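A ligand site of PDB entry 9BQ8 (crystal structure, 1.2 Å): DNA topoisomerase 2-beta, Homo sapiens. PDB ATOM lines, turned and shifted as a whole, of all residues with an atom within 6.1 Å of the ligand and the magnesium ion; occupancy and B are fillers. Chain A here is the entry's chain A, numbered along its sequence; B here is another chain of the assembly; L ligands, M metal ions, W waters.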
ATOM      1  N   GLU A  62      -3.063 -15.756  16.175  1.00  0.00           N
ATOM      2  CA  GLU A  62      -2.143 -15.138  15.227  1.00  0.00           C
ATOM      3  C   GLU A  62      -1.625 -16.167  14.227  1.00  0.00           C
ATOM      4  O   GLU A  62      -1.536 -15.888  13.016  1.00  0.00           O
ATOM      5  CB  GLU A  62      -0.970 -14.474  15.957  1.00  0.00           C
ATOM      6  CG  GLU A  62      -1.315 -13.253  16.809  1.00  0.00           C
ATOM      7  CD  GLU A  62      -1.754 -12.024  16.014  1.00  0.00           C
ATOM      8  OE1 GLU A  62      -1.808 -12.050  14.770  1.00  0.00           O
ATOM      9  OE2 GLU A  62      -2.084 -10.993  16.643  1.00  0.00           O
ATOM     10  N   ILE A  63      -1.257 -17.346  14.710  1.00  0.00           N
ATOM     11  CA  ILE A  63      -0.719 -18.358  13.805  1.00  0.00           C
ATOM     12  C   ILE A  63      -1.824 -18.909  12.904  1.00  0.00           C
ATOM     13  O   ILE A  63      -1.592 -19.187  11.724  1.00  0.00           O
ATOM     14  CB  ILE A  63      -0.020 -19.461  14.621  1.00  0.00           C
ATOM     15  CG1 ILE A  63       1.089 -18.874  15.513  1.00  0.00           C
ATOM     16  CG2 ILE A  63       0.534 -20.534  13.697  1.00  0.00           C
ATOM     17  CD1 ILE A  63       2.102 -17.980  14.790  1.00  0.00           C
ATOM     18  N   VAL A  65      -4.611 -17.349  11.795  1.00  0.00           N
ATOM     19  CA  VAL A  65      -4.940 -16.389  10.741  1.00  0.00           C
ATOM     20  C   VAL A  65      -3.808 -16.311   9.715  1.00  0.00           C
ATOM     21  O   VAL A  65      -4.054 -16.137   8.518  1.00  0.00           O
ATOM     22  CB  VAL A  65      -5.290 -15.018  11.346  1.00  0.00           C
ATOM     23  CG1 VAL A  65      -5.485 -13.972  10.273  1.00  0.00           C
ATOM     24  CG2 VAL A  65      -6.545 -15.126  12.203  1.00  0.00           C
ATOM     25  N   ASN A  66      -2.551 -16.443  10.155  1.00  0.00           N
ATOM     26  CA  ASN A  66      -1.444 -16.480   9.194  1.00  0.00           C
ATOM     27  C   ASN A  66      -1.626 -17.631   8.201  1.00  0.00           C
ATOM     28  O   ASN A  66      -1.280 -17.496   7.022  1.00  0.00           O
ATOM     29  CB  ASN A  66      -0.115 -16.647   9.918  1.00  0.00           C
ATOM     30  CG  ASN A  66       0.385 -15.361  10.512  1.00  0.00           C
ATOM     31  OD1 ASN A  66      -0.114 -14.271  10.209  1.00  0.00           O
ATOM     32  ND2 ASN A  66       1.401 -15.474  11.368  1.00  0.00           N
ATOM     33  N   ALA A  67      -2.092 -18.786   8.676  1.00  0.00           N
ATOM     34  CA  ALA A  67      -2.334 -19.907   7.779  1.00  0.00           C
ATOM     35  C   ALA A  67      -3.447 -19.584   6.795  1.00  0.00           C
ATOM     36  O   ALA A  67      -3.301 -19.821   5.588  1.00  0.00           O
ATOM     37  CB  ALA A  67      -2.651 -21.169   8.580  1.00  0.00           C
ATOM     38  N   ASP A  69      -4.248 -16.703   5.777  1.00  0.00           N
ATOM     39  CA  ASP A  69      -3.736 -15.681   4.878  1.00  0.00           C
ATOM     40  C   ASP A  69      -2.987 -16.289   3.696  1.00  0.00           C
ATOM     41  O   ASP A  69      -2.878 -15.651   2.648  1.00  0.00           O
ATOM     42  CB  ASP A  69      -2.771 -14.761   5.627  1.00  0.00           C
ATOM     43  CG  ASP A  69      -3.490 -13.728   6.480  1.00  0.00           C
ATOM     44  OD1 ASP A  69      -4.718 -13.571   6.347  1.00  0.00           O
ATOM     45  OD2 ASP A  69      -2.796 -13.055   7.278  1.00  0.00           O
ATOM     46  N   ASN A  70      -2.442 -17.503   3.859  1.00  0.00           N
ATOM     47  CA  ASN A  70      -1.712 -18.098   2.748  1.00  0.00           C
ATOM     48  C   ASN A  70      -2.623 -18.422   1.575  1.00  0.00           C
ATOM     49  O   ASN A  70      -2.127 -18.566   0.450  1.00  0.00           O
ATOM     50  CB  ASN A  70      -0.941 -19.337   3.173  1.00  0.00           C
ATOM     51  CG  ASN A  70       0.234 -19.617   2.262  1.00  0.00           C
ATOM     52  OD1 ASN A  70       1.093 -18.756   2.079  1.00  0.00           O
ATOM     53  ND2 ASN A  70       0.254 -20.804   1.648  1.00  0.00           N
ATOM     54  N   ARG A  73      -1.980 -15.750  -0.775  1.00  0.00           N
ATOM     55  CA  ARG A  73      -0.708 -15.883  -1.487  1.00  0.00           C
ATOM     56  C   ARG A  73      -0.774 -16.968  -2.540  1.00  0.00           C
ATOM     57  O   ARG A  73      -0.062 -16.900  -3.555  1.00  0.00           O
ATOM     58  CB  ARG A  73       0.408 -16.258  -0.510  1.00  0.00           C
ATOM     59  CG  ARG A  73       1.177 -15.111   0.091  1.00  0.00           C
ATOM     60  CD  ARG A  73       2.348 -15.640   0.927  1.00  0.00           C
ATOM     61  NE  ARG A  73       3.493 -16.043   0.100  1.00  0.00           N
ATOM     62  CZ  ARG A  73       4.038 -17.255   0.072  1.00  0.00           C
ATOM     63  NH1 ARG A  73       3.570 -18.257   0.800  1.00  0.00           N
ATOM     64  NH2 ARG A  73       5.089 -17.469  -0.724  1.00  0.00           N
ATOM     65  N   ASN A  95      -0.231 -25.776   6.995  1.00  0.00           N
ATOM     66  CA  ASN A  95      -0.997 -25.414   5.808  1.00  0.00           C
ATOM     67  C   ASN A  95      -0.242 -25.832   4.565  1.00  0.00           C
ATOM     68  O   ASN A  95       0.986 -25.949   4.583  1.00  0.00           O
ATOM     69  CB  ASN A  95      -1.313 -23.914   5.778  1.00  0.00           C
ATOM     70  CG  ASN A  95      -0.078 -23.050   5.574  1.00  0.00           C
ATOM     71  OD1 ASN A  95       0.525 -22.562   6.538  1.00  0.00           O
ATOM     72  ND2 ASN A  95       0.297 -22.851   4.325  1.00  0.00           N
ATOM     73  N   LYS A  98       1.716 -22.522  -1.329  1.00  0.00           N
ATOM     74  CA  LYS A  98       3.115 -22.103  -1.415  1.00  0.00           C
ATOM     75  C   LYS A  98       3.722 -21.917  -0.029  1.00  0.00           C
ATOM     76  O   LYS A  98       3.125 -21.315   0.867  1.00  0.00           O
ATOM     77  CB  LYS A  98       3.219 -20.788  -2.175  1.00  0.00           C
ATOM     78  CG  LYS A  98       3.295 -20.937  -3.672  1.00  0.00           C
ATOM     79  CD  LYS A  98       3.830 -19.680  -4.358  1.00  0.00           C
ATOM     80  CE  LYS A  98       5.288 -19.355  -3.991  1.00  0.00           C
ATOM     81  NZ  LYS A  98       6.315 -20.290  -4.555  1.00  0.00           N
ATOM     82  N   GLY A  99       4.947 -22.414   0.120  1.00  0.00           N
ATOM     83  CA  GLY A  99       5.747 -22.160   1.293  1.00  0.00           C
ATOM     84  C   GLY A  99       6.395 -20.800   1.220  1.00  0.00           C
ATOM     85  O   GLY A  99       6.081 -19.970   0.359  1.00  0.00           O
ATOM     86  N   ILE A 100       7.310 -20.565   2.143  1.00  0.00           N
ATOM     87  CA  ILE A 100       8.025 -19.284   2.245  1.00  0.00           C
ATOM     88  C   ILE A 100       9.375 -19.446   1.559  1.00  0.00           C
ATOM     89  O   ILE A 100      10.070 -20.455   1.813  1.00  0.00           O
ATOM     90  CB  ILE A 100       8.206 -18.868   3.715  1.00  0.00           C
ATOM     91  CG1 ILE A 100       6.850 -18.729   4.395  1.00  0.00           C
ATOM     92  CG2 ILE A 100       8.965 -17.558   3.793  1.00  0.00           C
ATOM     93  CD1 ILE A 100       6.937 -18.742   5.900  1.00  0.00           C
ATOM     94  N   ILE A 116      11.166 -13.116   9.222  1.00  0.00           N
ATOM     95  CA  ILE A 116       9.762 -12.792   9.421  1.00  0.00           C
ATOM     96  C   ILE A 116       9.142 -13.542  10.597  1.00  0.00           C
ATOM     97  O   ILE A 116       8.042 -13.182  11.028  1.00  0.00           O
ATOM     98  CB  ILE A 116       8.962 -12.940   8.112  1.00  0.00           C
ATOM     99  CG1 ILE A 116       8.819 -14.410   7.713  1.00  0.00           C
ATOM    100  CG2 ILE A 116       9.608 -12.111   7.004  1.00  0.00           C
ATOM    101  CD1 ILE A 116       8.192 -14.626   6.330  1.00  0.00           C
ATOM    102  N   PHE A 117       9.832 -14.525  11.167  1.00  0.00           N
ATOM    103  CA  PHE A 117       9.407 -15.135  12.418  1.00  0.00           C
ATOM    104  C   PHE A 117      10.252 -14.742  13.614  1.00  0.00           C
ATOM    105  O   PHE A 117       9.828 -14.982  14.754  1.00  0.00           O
ATOM    106  CB  PHE A 117       9.364 -16.665  12.287  1.00  0.00           C
ATOM    107  CG  PHE A 117       8.221 -17.156  11.450  1.00  0.00           C
ATOM    108  CD1 PHE A 117       6.984 -17.390  12.035  1.00  0.00           C
ATOM    109  CD2 PHE A 117       8.362 -17.338  10.088  1.00  0.00           C
ATOM    110  CE1 PHE A 117       5.920 -17.823  11.275  1.00  0.00           C
ATOM    111  CE2 PHE A 117       7.298 -17.772   9.329  1.00  0.00           C
ATOM    112  CZ  PHE A 117       6.078 -18.018   9.926  1.00  0.00           C
ATOM    113  N   THR A 122       8.157  -7.115  10.723  1.00  0.00           N
ATOM    114  CA  THR A 122       8.510  -7.762   9.465  1.00  0.00           C
ATOM    115  C   THR A 122       7.248  -8.385   8.875  1.00  0.00           C
ATOM    116  O   THR A 122       6.490  -9.056   9.587  1.00  0.00           O
ATOM    117  CB  THR A 122       9.578  -8.841   9.684  1.00  0.00           C
ATOM    118  OG1 THR A 122       9.163  -9.760  10.715  1.00  0.00           O
ATOM    119  CG2 THR A 122      10.930  -8.214  10.065  1.00  0.00           C
ATOM    120  N   SER A 123       7.027  -8.162   7.580  1.00  0.00           N
ATOM    121  CA  SER A 123       5.740  -8.497   7.002  1.00  0.00           C
ATOM    122  C   SER A 123       5.829  -8.474   5.483  1.00  0.00           C
ATOM    123  O   SER A 123       6.624  -7.733   4.912  1.00  0.00           O
ATOM    124  CB  SER A 123       4.688  -7.472   7.448  1.00  0.00           C
ATOM    125  OG  SER A 123       3.381  -7.789   6.987  1.00  0.00           O
ATOM    126  N   SER A 124       4.972  -9.269   4.841  1.00  0.00           N
ATOM    127  CA  SER A 124       4.674  -9.115   3.429  1.00  0.00           C
ATOM    128  C   SER A 124       3.433  -8.257   3.192  1.00  0.00           C
ATOM    129  O   SER A 124       2.990  -8.130   2.049  1.00  0.00           O
ATOM    130  CB  SER A 124       4.512 -10.474   2.764  1.00  0.00           C
ATOM    131  OG  SER A 124       3.468 -11.223   3.352  1.00  0.00           O
ATOM    132  N   ASN A 125       2.874  -7.669   4.246  1.00  0.00           N
ATOM    133  CA  ASN A 125       1.630  -6.916   4.175  1.00  0.00           C
ATOM    134  C   ASN A 125       1.822  -5.418   4.382  1.00  0.00           C
ATOM    135  O   ASN A 125       0.869  -4.733   4.752  1.00  0.00           O
ATOM    136  CB  ASN A 125       0.620  -7.458   5.184  1.00  0.00           C
ATOM    137  CG  ASN A 125       0.135  -8.819   4.807  1.00  0.00           C
ATOM    138  OD1 ASN A 125      -0.528  -8.965   3.788  1.00  0.00           O
ATOM    139  ND2 ASN A 125       0.446  -9.824   5.617  1.00  0.00           N
ATOM    140  N   GLY A 135      -5.694 -11.024   6.605  1.00  0.00           N
ATOM    141  CA  GLY A 135      -5.870 -10.495   7.937  1.00  0.00           C
ATOM    142  C   GLY A 135      -4.617  -9.831   8.484  1.00  0.00           C
ATOM    143  O   GLY A 135      -4.703  -8.919   9.297  1.00  0.00           O
ATOM    144  N   GLY A 136      -3.449 -10.284   8.034  1.00  0.00           N
ATOM    145  CA  GLY A 136      -2.209  -9.709   8.501  1.00  0.00           C
ATOM    146  C   GLY A 136      -2.009  -8.295   7.992  1.00  0.00           C
ATOM    147  O   GLY A 136      -2.226  -7.994   6.811  1.00  0.00           O
ATOM    148  N   ARG A 137      -1.571  -7.416   8.898  1.00  0.00           N
ATOM    149  CA  ARG A 137      -1.355  -5.999   8.596  1.00  0.00           C
ATOM    150  C   ARG A 137      -0.099  -5.428   9.221  1.00  0.00           C
ATOM    151  O   ARG A 137       0.489  -4.514   8.634  1.00  0.00           O
ATOM    152  CB  ARG A 137      -2.547  -5.149   9.074  1.00  0.00           C
ATOM    153  CG  ARG A 137      -3.916  -5.614   8.613  1.00  0.00           C
ATOM    154  CD  ARG A 137      -4.131  -5.376   7.123  1.00  0.00           C
ATOM    155  NE  ARG A 137      -4.133  -3.951   6.806  1.00  0.00           N
ATOM    156  CZ  ARG A 137      -3.402  -3.363   5.871  1.00  0.00           C
ATOM    157  NH1 ARG A 137      -2.670  -4.063   5.021  1.00  0.00           N
ATOM    158  NH2 ARG A 137      -3.423  -2.037   5.769  1.00  0.00           N
ATOM    159  N   ASN A 138       0.323  -5.888  10.404  1.00  0.00           N
ATOM    160  CA  ASN A 138       1.236  -5.109  11.227  1.00  0.00           C
ATOM    161  C   ASN A 138       2.659  -5.643  11.340  1.00  0.00           C
ATOM    162  O   ASN A 138       3.537  -4.894  11.769  1.00  0.00           O
ATOM    163  CB  ASN A 138       0.659  -4.954  12.629  1.00  0.00           C
ATOM    164  CG  ASN A 138      -0.699  -4.328  12.601  1.00  0.00           C
ATOM    165  OD1 ASN A 138      -0.954  -3.442  11.779  1.00  0.00           O
ATOM    166  ND2 ASN A 138      -1.585  -4.782  13.473  1.00  0.00           N
ATOM    167  N   GLY A 139       2.906  -6.912  11.018  1.00  0.00           N
ATOM    168  CA  GLY A 139       4.241  -7.471  11.154  1.00  0.00           C
ATOM    169  C   GLY A 139       4.627  -7.876  12.562  1.00  0.00           C
ATOM    170  O   GLY A 139       5.828  -7.917  12.864  1.00  0.00           O
ATOM    171  N   TYR A 140       3.650  -8.197  13.411  1.00  0.00           N
ATOM    172  CA  TYR A 140       3.874  -8.600  14.787  1.00  0.00           C
ATOM    173  C   TYR A 140       3.475 -10.033  15.099  1.00  0.00           C
ATOM    174  O   TYR A 140       4.167 -10.700  15.880  1.00  0.00           O
ATOM    175  CB  TYR A 140       3.072  -7.701  15.740  1.00  0.00           C
ATOM    176  CG  TYR A 140       3.782  -6.483  16.267  1.00  0.00           C
ATOM    177  CD1 TYR A 140       4.952  -6.596  17.007  1.00  0.00           C
ATOM    178  CD2 TYR A 140       3.236  -5.224  16.118  1.00  0.00           C
ATOM    179  CE1 TYR A 140       5.575  -5.486  17.521  1.00  0.00           C
ATOM    180  CE2 TYR A 140       3.851  -4.093  16.641  1.00  0.00           C
ATOM    181  CZ  TYR A 140       5.026  -4.241  17.346  1.00  0.00           C
ATOM    182  OH  TYR A 140       5.649  -3.131  17.861  1.00  0.00           O
ATOM    183  N   GLY A 141       2.340 -10.506  14.567  1.00  0.00           N
ATOM    184  CA  GLY A 141       1.646 -11.652  15.154  1.00  0.00           C
ATOM    185  C   GLY A 141       2.514 -12.870  15.412  1.00  0.00           C
ATOM    186  O   GLY A 141       2.458 -13.464  16.503  1.00  0.00           O
ATOM    187  N   ALA A 142       3.300 -13.287  14.428  1.00  0.00           N
ATOM    188  CA  ALA A 142       4.101 -14.504  14.575  1.00  0.00           C
ATOM    189  C   ALA A 142       5.208 -14.321  15.604  1.00  0.00           C
ATOM    190  O   ALA A 142       5.539 -15.268  16.339  1.00  0.00           O
ATOM    191  CB  ALA A 142       4.699 -14.924  13.241  1.00  0.00           C
ATOM    192  N   LYS A 143       5.800 -13.133  15.659  1.00  0.00           N
ATOM    193  CA  LYS A 143       6.823 -12.856  16.655  1.00  0.00           C
ATOM    194  C   LYS A 143       6.218 -12.835  18.047  1.00  0.00           C
ATOM    195  O   LYS A 143       6.859 -13.279  19.019  1.00  0.00           O
ATOM    196  CB  LYS A 143       7.521 -11.529  16.373  1.00  0.00           C
ATOM    197  CG  LYS A 143       8.632 -11.600  15.324  1.00  0.00           C
ATOM    198  CD  LYS A 143       8.107 -11.829  13.894  1.00  0.00           C
ATOM    199  CE  LYS A 143       7.329 -10.634  13.361  1.00  0.00           C
ATOM    200  NZ  LYS A 143       6.838 -10.833  11.979  1.00  0.00           N
ATOM    201  N   THR A 156       9.167 -24.827   6.797  1.00  0.00           N
ATOM    202  CA  THR A 156       8.533 -24.421   5.553  1.00  0.00           C
ATOM    203  C   THR A 156       9.322 -25.021   4.412  1.00  0.00           C
ATOM    204  O   THR A 156      10.533 -25.219   4.509  1.00  0.00           O
ATOM    205  CB  THR A 156       8.386 -22.894   5.471  1.00  0.00           C
ATOM    206  OG1 THR A 156       7.558 -22.533   4.352  1.00  0.00           O
ATOM    207  CG2 THR A 156       9.739 -22.199   5.348  1.00  0.00           C
ATOM    208  N   THR A 190       3.797 -25.154   5.115  1.00  0.00           N
ATOM    209  CA  THR A 190       4.388 -24.494   6.268  1.00  0.00           C
ATOM    210  C   THR A 190       3.761 -25.101   7.510  1.00  0.00           C
ATOM    211  O   THR A 190       2.551 -25.358   7.541  1.00  0.00           O
ATOM    212  CB  THR A 190       4.185 -22.966   6.242  1.00  0.00           C
ATOM    213  OG1 THR A 190       4.908 -22.413   5.137  1.00  0.00           O
ATOM    214  CG2 THR A 190       4.676 -22.324   7.538  1.00  0.00           C
ATOM    215  N   ILE A 192       3.916 -24.530  11.786  1.00  0.00           N
ATOM    216  CA  ILE A 192       4.363 -23.804  12.962  1.00  0.00           C
ATOM    217  C   ILE A 192       3.990 -24.645  14.167  1.00  0.00           C
ATOM    218  O   ILE A 192       2.809 -24.964  14.370  1.00  0.00           O
ATOM    219  CB  ILE A 192       3.693 -22.420  13.053  1.00  0.00           C
ATOM    220  CG1 ILE A 192       3.867 -21.638  11.738  1.00  0.00           C
ATOM    221  CG2 ILE A 192       4.213 -21.655  14.264  1.00  0.00           C
ATOM    222  CD1 ILE A 192       5.298 -21.470  11.273  1.00  0.00           C
ATOM    223  N   GLN A 351      -3.769  -4.479  17.982  1.00  0.00           N
ATOM    224  CA  GLN A 351      -3.204  -5.670  17.374  1.00  0.00           C
ATOM    225  C   GLN A 351      -4.147  -6.867  17.511  1.00  0.00           C
ATOM    226  O   GLN A 351      -4.092  -7.778  16.678  1.00  0.00           O
ATOM    227  CB  GLN A 351      -1.859  -5.991  18.035  1.00  0.00           C
ATOM    228  CG  GLN A 351      -1.199  -7.279  17.579  1.00  0.00           C
ATOM    229  CD  GLN A 351      -0.727  -7.253  16.134  1.00  0.00           C
ATOM    230  OE1 GLN A 351      -0.332  -6.206  15.614  1.00  0.00           O
ATOM    231  NE2 GLN A 351      -0.767  -8.402  15.473  1.00  0.00           N
ATOM    232  N   LYS A 353      -7.269  -6.967  16.988  1.00  0.00           N
ATOM    233  CA  LYS A 353      -8.167  -6.957  15.817  1.00  0.00           C
ATOM    234  C   LYS A 353      -9.593  -7.392  16.144  1.00  0.00           C
ATOM    235  O   LYS A 353     -10.271  -7.988  15.303  1.00  0.00           O
ATOM    236  CB  LYS A 353      -7.600  -7.787  14.660  1.00  0.00           C
ATOM    237  CG  LYS A 353      -6.257  -7.300  14.179  1.00  0.00           C
ATOM    238  CD  LYS A 353      -5.692  -8.247  13.149  1.00  0.00           C
ATOM    239  CE  LYS A 353      -4.226  -7.964  12.922  1.00  0.00           C
ATOM    240  NZ  LYS A 353      -3.655  -8.910  11.933  1.00  0.00           N
ATOM    241  N   TYR B   9       9.076  -8.965   1.292  1.00  0.00           N
ATOM    242  CA  TYR B   9       9.299  -9.153   2.716  1.00  0.00           C
ATOM    243  C   TYR B   9      10.091  -7.956   3.249  1.00  0.00           C
ATOM    244  O   TYR B   9      11.273  -7.797   2.938  1.00  0.00           O
ATOM    245  CB  TYR B   9      10.024 -10.471   2.979  1.00  0.00           C
ATOM    246  CG  TYR B   9       9.207 -11.651   2.523  1.00  0.00           C
ATOM    247  CD1 TYR B   9       8.166 -12.140   3.299  1.00  0.00           C
ATOM    248  CD2 TYR B   9       9.466 -12.280   1.315  1.00  0.00           C
ATOM    249  CE1 TYR B   9       7.414 -13.207   2.893  1.00  0.00           C
ATOM    250  CE2 TYR B   9       8.720 -13.352   0.904  1.00  0.00           C
ATOM    251  CZ  TYR B   9       7.695 -13.819   1.696  1.00  0.00           C
ATOM    252  OH  TYR B   9       6.928 -14.887   1.292  1.00  0.00           O
HETATM  253  P1  LIG L   1       0.043  -9.156  11.776  1.00  0.00           P
HETATM  254  O1  LIG L   1      -0.354 -10.582  11.914  1.00  0.00           O
HETATM  255  O2  LIG L   1       0.998  -8.677  12.891  1.00  0.00           O
HETATM  256  O3  LIG L   1      -1.141  -8.153  11.606  1.00  0.00           O
HETATM  257  P2  LIG L   1       1.572 -10.280   9.477  1.00  0.00           P
HETATM  258  O4  LIG L   1       0.700 -11.491   9.362  1.00  0.00           O
HETATM  259  O5  LIG L   1       2.028  -9.768   8.100  1.00  0.00           O
HETATM  260  N1  LIG L   1       0.832  -8.999  10.260  1.00  0.00           N
HETATM  261  P3  LIG L   1       3.205 -11.978  11.103  1.00  0.00           P
HETATM  262  O6  LIG L   1       4.233 -11.693  12.132  1.00  0.00           O
HETATM  263  O7  LIG L   1       1.927 -12.644  11.597  1.00  0.00           O
HETATM  264  O8  LIG L   1       2.809 -10.604  10.378  1.00  0.00           O
HETATM  265  O9  LIG L   1       3.810 -12.852   9.938  1.00  0.00           O
HETATM  266  C1  LIG L   1       5.015 -12.368   9.303  1.00  0.00           C
HETATM  267  C2  LIG L   1       5.031 -12.789   7.856  1.00  0.00           C
HETATM  268  O10 LIG L   1       5.302 -14.194   7.775  1.00  0.00           O
HETATM  269  C3  LIG L   1       3.724 -12.611   7.096  1.00  0.00           C
HETATM  270  O11 LIG L   1       3.607 -11.282   6.589  1.00  0.00           O
HETATM  271  C4  LIG L   1       3.863 -13.629   5.965  1.00  0.00           C
HETATM  272  O12 LIG L   1       4.636 -13.107   4.891  1.00  0.00           O
HETATM  273  C5  LIG L   1       4.670 -14.742   6.638  1.00  0.00           C
HETATM  274  N2  LIG L   1       3.896 -15.905   7.060  1.00  0.00           N
HETATM  275  C6  LIG L   1       3.436 -16.181   8.326  1.00  0.00           C
HETATM  276  N3  LIG L   1       2.805 -17.326   8.416  1.00  0.00           N
HETATM  277  C7  LIG L   1       2.852 -17.844   7.134  1.00  0.00           C
HETATM  278  C8  LIG L   1       2.355 -19.028   6.565  1.00  0.00           C
HETATM  279  N4  LIG L   1       1.666 -19.942   7.244  1.00  0.00           N
HETATM  280  N5  LIG L   1       2.591 -19.241   5.251  1.00  0.00           N
HETATM  281  C9  LIG L   1       3.263 -18.315   4.561  1.00  0.00           C
HETATM  282  N6  LIG L   1       3.777 -17.164   4.986  1.00  0.00           N
HETATM  283  C10 LIG L   1       3.534 -16.974   6.293  1.00  0.00           C
HETATM  284 MG    MG M   1      -0.068 -12.395  11.062  1.00  0.00          MG
HETATM  285  O   HOH W   1       0.951 -15.968   3.490  1.00  0.00           O
HETATM  286  O   HOH W   2      -0.079 -13.031   7.055  1.00  0.00           O
HETATM  287  O   HOH W   3       2.498 -18.236  11.147  1.00  0.00           O
HETATM  288  O   HOH W   4      -0.652 -13.323  12.785  1.00  0.00           O
HETATM  289  O   HOH W   5       4.866 -15.493   2.908  1.00  0.00           O
HETATM  290  O   HOH W   6       0.703 -20.170  10.169  1.00  0.00           O
HETATM  291  O   HOH W   7       2.857 -21.537   3.650  1.00  0.00           O
HETATM  292  O   HOH W   8      -2.089 -12.340  10.312  1.00  0.00           O
HETATM  293  O   HOH W   9       0.650 -15.618   6.219  1.00  0.00           O
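N of Gly 139 lies within hydrogen-bond range of O2 of the ligand, at 3.2 Å.
OG of Ser 124 lies within hydrogen-bond range of O12 of the ligand, 2.7 Å away.
O11 of the ligand sits at hydrogen-bond distance from N of Ser 124, at 3.0 Å.
NE2 of Gln 351 is in hydrogen-bond range of O2 of the ligand, 3.1 Å away.
An oxygen (O3) of the ligand is in hydrogen-bond range of the backbone NH (N) of Arg 137 (2.8 Å).
ND2 of Asn 125 lies within hydrogen-bond range of O5 of the ligand (2.9 Å).
O3 of the ligand lies within hydrogen-bond range of N of Asn 138 (3.0 Å).
An oxygen (O2) of the ligand is in hydrogen-bond range of the backbone NH of Gly 141, at 2.8 Å.
N of Ala 142 sits at hydrogen-bond distance from O6 of the ligand (2.9 Å).
N of Tyr 140 sits at hydrogen-bond distance from O2 of the ligand (2.7 Å).
An oxygen (O3) of the ligand is in salt-bridge range of the side-chain amino group of Lys 353, at 2.6 Å.
A nitrogen (N4) of the ligand lies within hydrogen-bond range of the side-chain amide oxygen of Asn 95, 2.9 Å away.
An oxygen (O5) of the ligand is in hydrogen-bond range of the side-chain hydroxyl (OG) of Ser 123 (2.6 Å).
NZ of Lys 143 lies within salt-bridge range of O6 of the ligand (2.7 Å).
The side-chain carboxylate (OE2) of Glu 62 sits at hydrogen-bond distance from the side-chain amide nitrogen (NE2) of Gln 351, 3.1 Å away.
ND2 of Asn 66 sits close to O of Glu 62 (3.4 Å).
The side-chain carboxylate (OD2) of Asp 69 sits at hydrogen-bond distance from the backbone NH (N) of Gly 136, at 2.9 Å.
The side-chain amide nitrogen of Asn 138 sits at hydrogen-bond distance from the side-chain amide oxygen of Gln 351.
The backbone carbonyl oxygen (O) of Thr 190 sits at hydrogen-bond distance from the backbone NH (N) of Asn 95, at 2.9 Å.
The side-chain hydroxyl (OG1) of Thr 122 is in hydrogen-bond range of the side-chain amino group (NZ) of Lys 143, 2.9 Å away.
The side-chain amide nitrogen of Asn 125 sits close to the backbone carbonyl oxygen of Gly 136 (3.5 Å).
The guanidinium group of Arg 73 lies within hydrogen-bond range of the backbone carbonyl oxygen of Lys 98 (3.1 Å).
OE1 of Glu 62 touches O1 of the ligand, at 3.5 Å.
Asn 70 touches the ligand (OD1 to C9, 3.3 Å).
NH1 of Arg 73 touches C9 of the ligand, 3.8 Å away.
Ile 100 touches the ligand.
Ile 116 touches the ligand (CD1 to O10, 3.3 Å).
CZ of Phe 117 touches C6 of the ligand (3.6 Å).
Thr 122 touches the ligand.
CA of Gly 136 touches O4 of the ligand, 3.5 Å away.
CG2 of Thr 190 touches N4 of the ligand (3.8 Å).
Tyr 9 of chain B touches the ligand (CE1 to O12, 3.4 Å).
Hydrophobic or aromatic side chains that line the ligand: Ile 100, Ile 116, Phe 117, Tyr 140, Ala 142 and Tyr 9 of chain B.
Of the 33 residues printed, 24 come within 4 Å of the ligand.
The nearest printed residue that does not touch the ligand is Ala 67 (4.04 Å).
Of the 33 residues printed, 1 comes within 4 Å of the magnesium ion.
The magnesium ion is bound by O1 of the ligand (2.0 Å), water W4 (2.0 Å), OD1 of Asn 66 (2.1 Å), O4 of the ligand (2.1 Å), O7 of the ligand (2.1 Å) and water W8 (2.2 Å).
The magnesium ion has six donor atoms within binding distance.
Water W4 lies within hydrogen-bond range of the side-chain carboxylate of Glu 62 (2.6 Å) and the side-chain amide nitrogen of Asn 66 (3.3 Å).
Water W7 lies within hydrogen-bond range of OG1 of Thr 190 (2.7 Å), O of Lys 98 (2.8 Å), N5 of the ligand (2.8 Å), ND2 of Asn 95 (3.0 Å) and ND2 of Asn 70 (3.4 Å).
Water W5 lies within hydrogen-bond range of the side-chain hydroxyl of Tyr 9 of chain B, a nitrogen (N6) of the ligand and the guanidinium group of Arg 73.
Water W3 bridges a nitrogen (N3) of the ligand (2.9 Å) and the side-chain amide nitrogen of Asn 66 (3.0 Å).
Water W6 lies within hydrogen-bond range of O of Ile 63 (2.9 Å), N4 of the ligand (3.1 Å) and N of Ala 67 (3.5 Å).
Water W1 lies within hydrogen-bond range of the side-chain amide oxygen of Asn 70 (3.1 Å) and a nitrogen (N6) of the ligand (3.4 Å).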
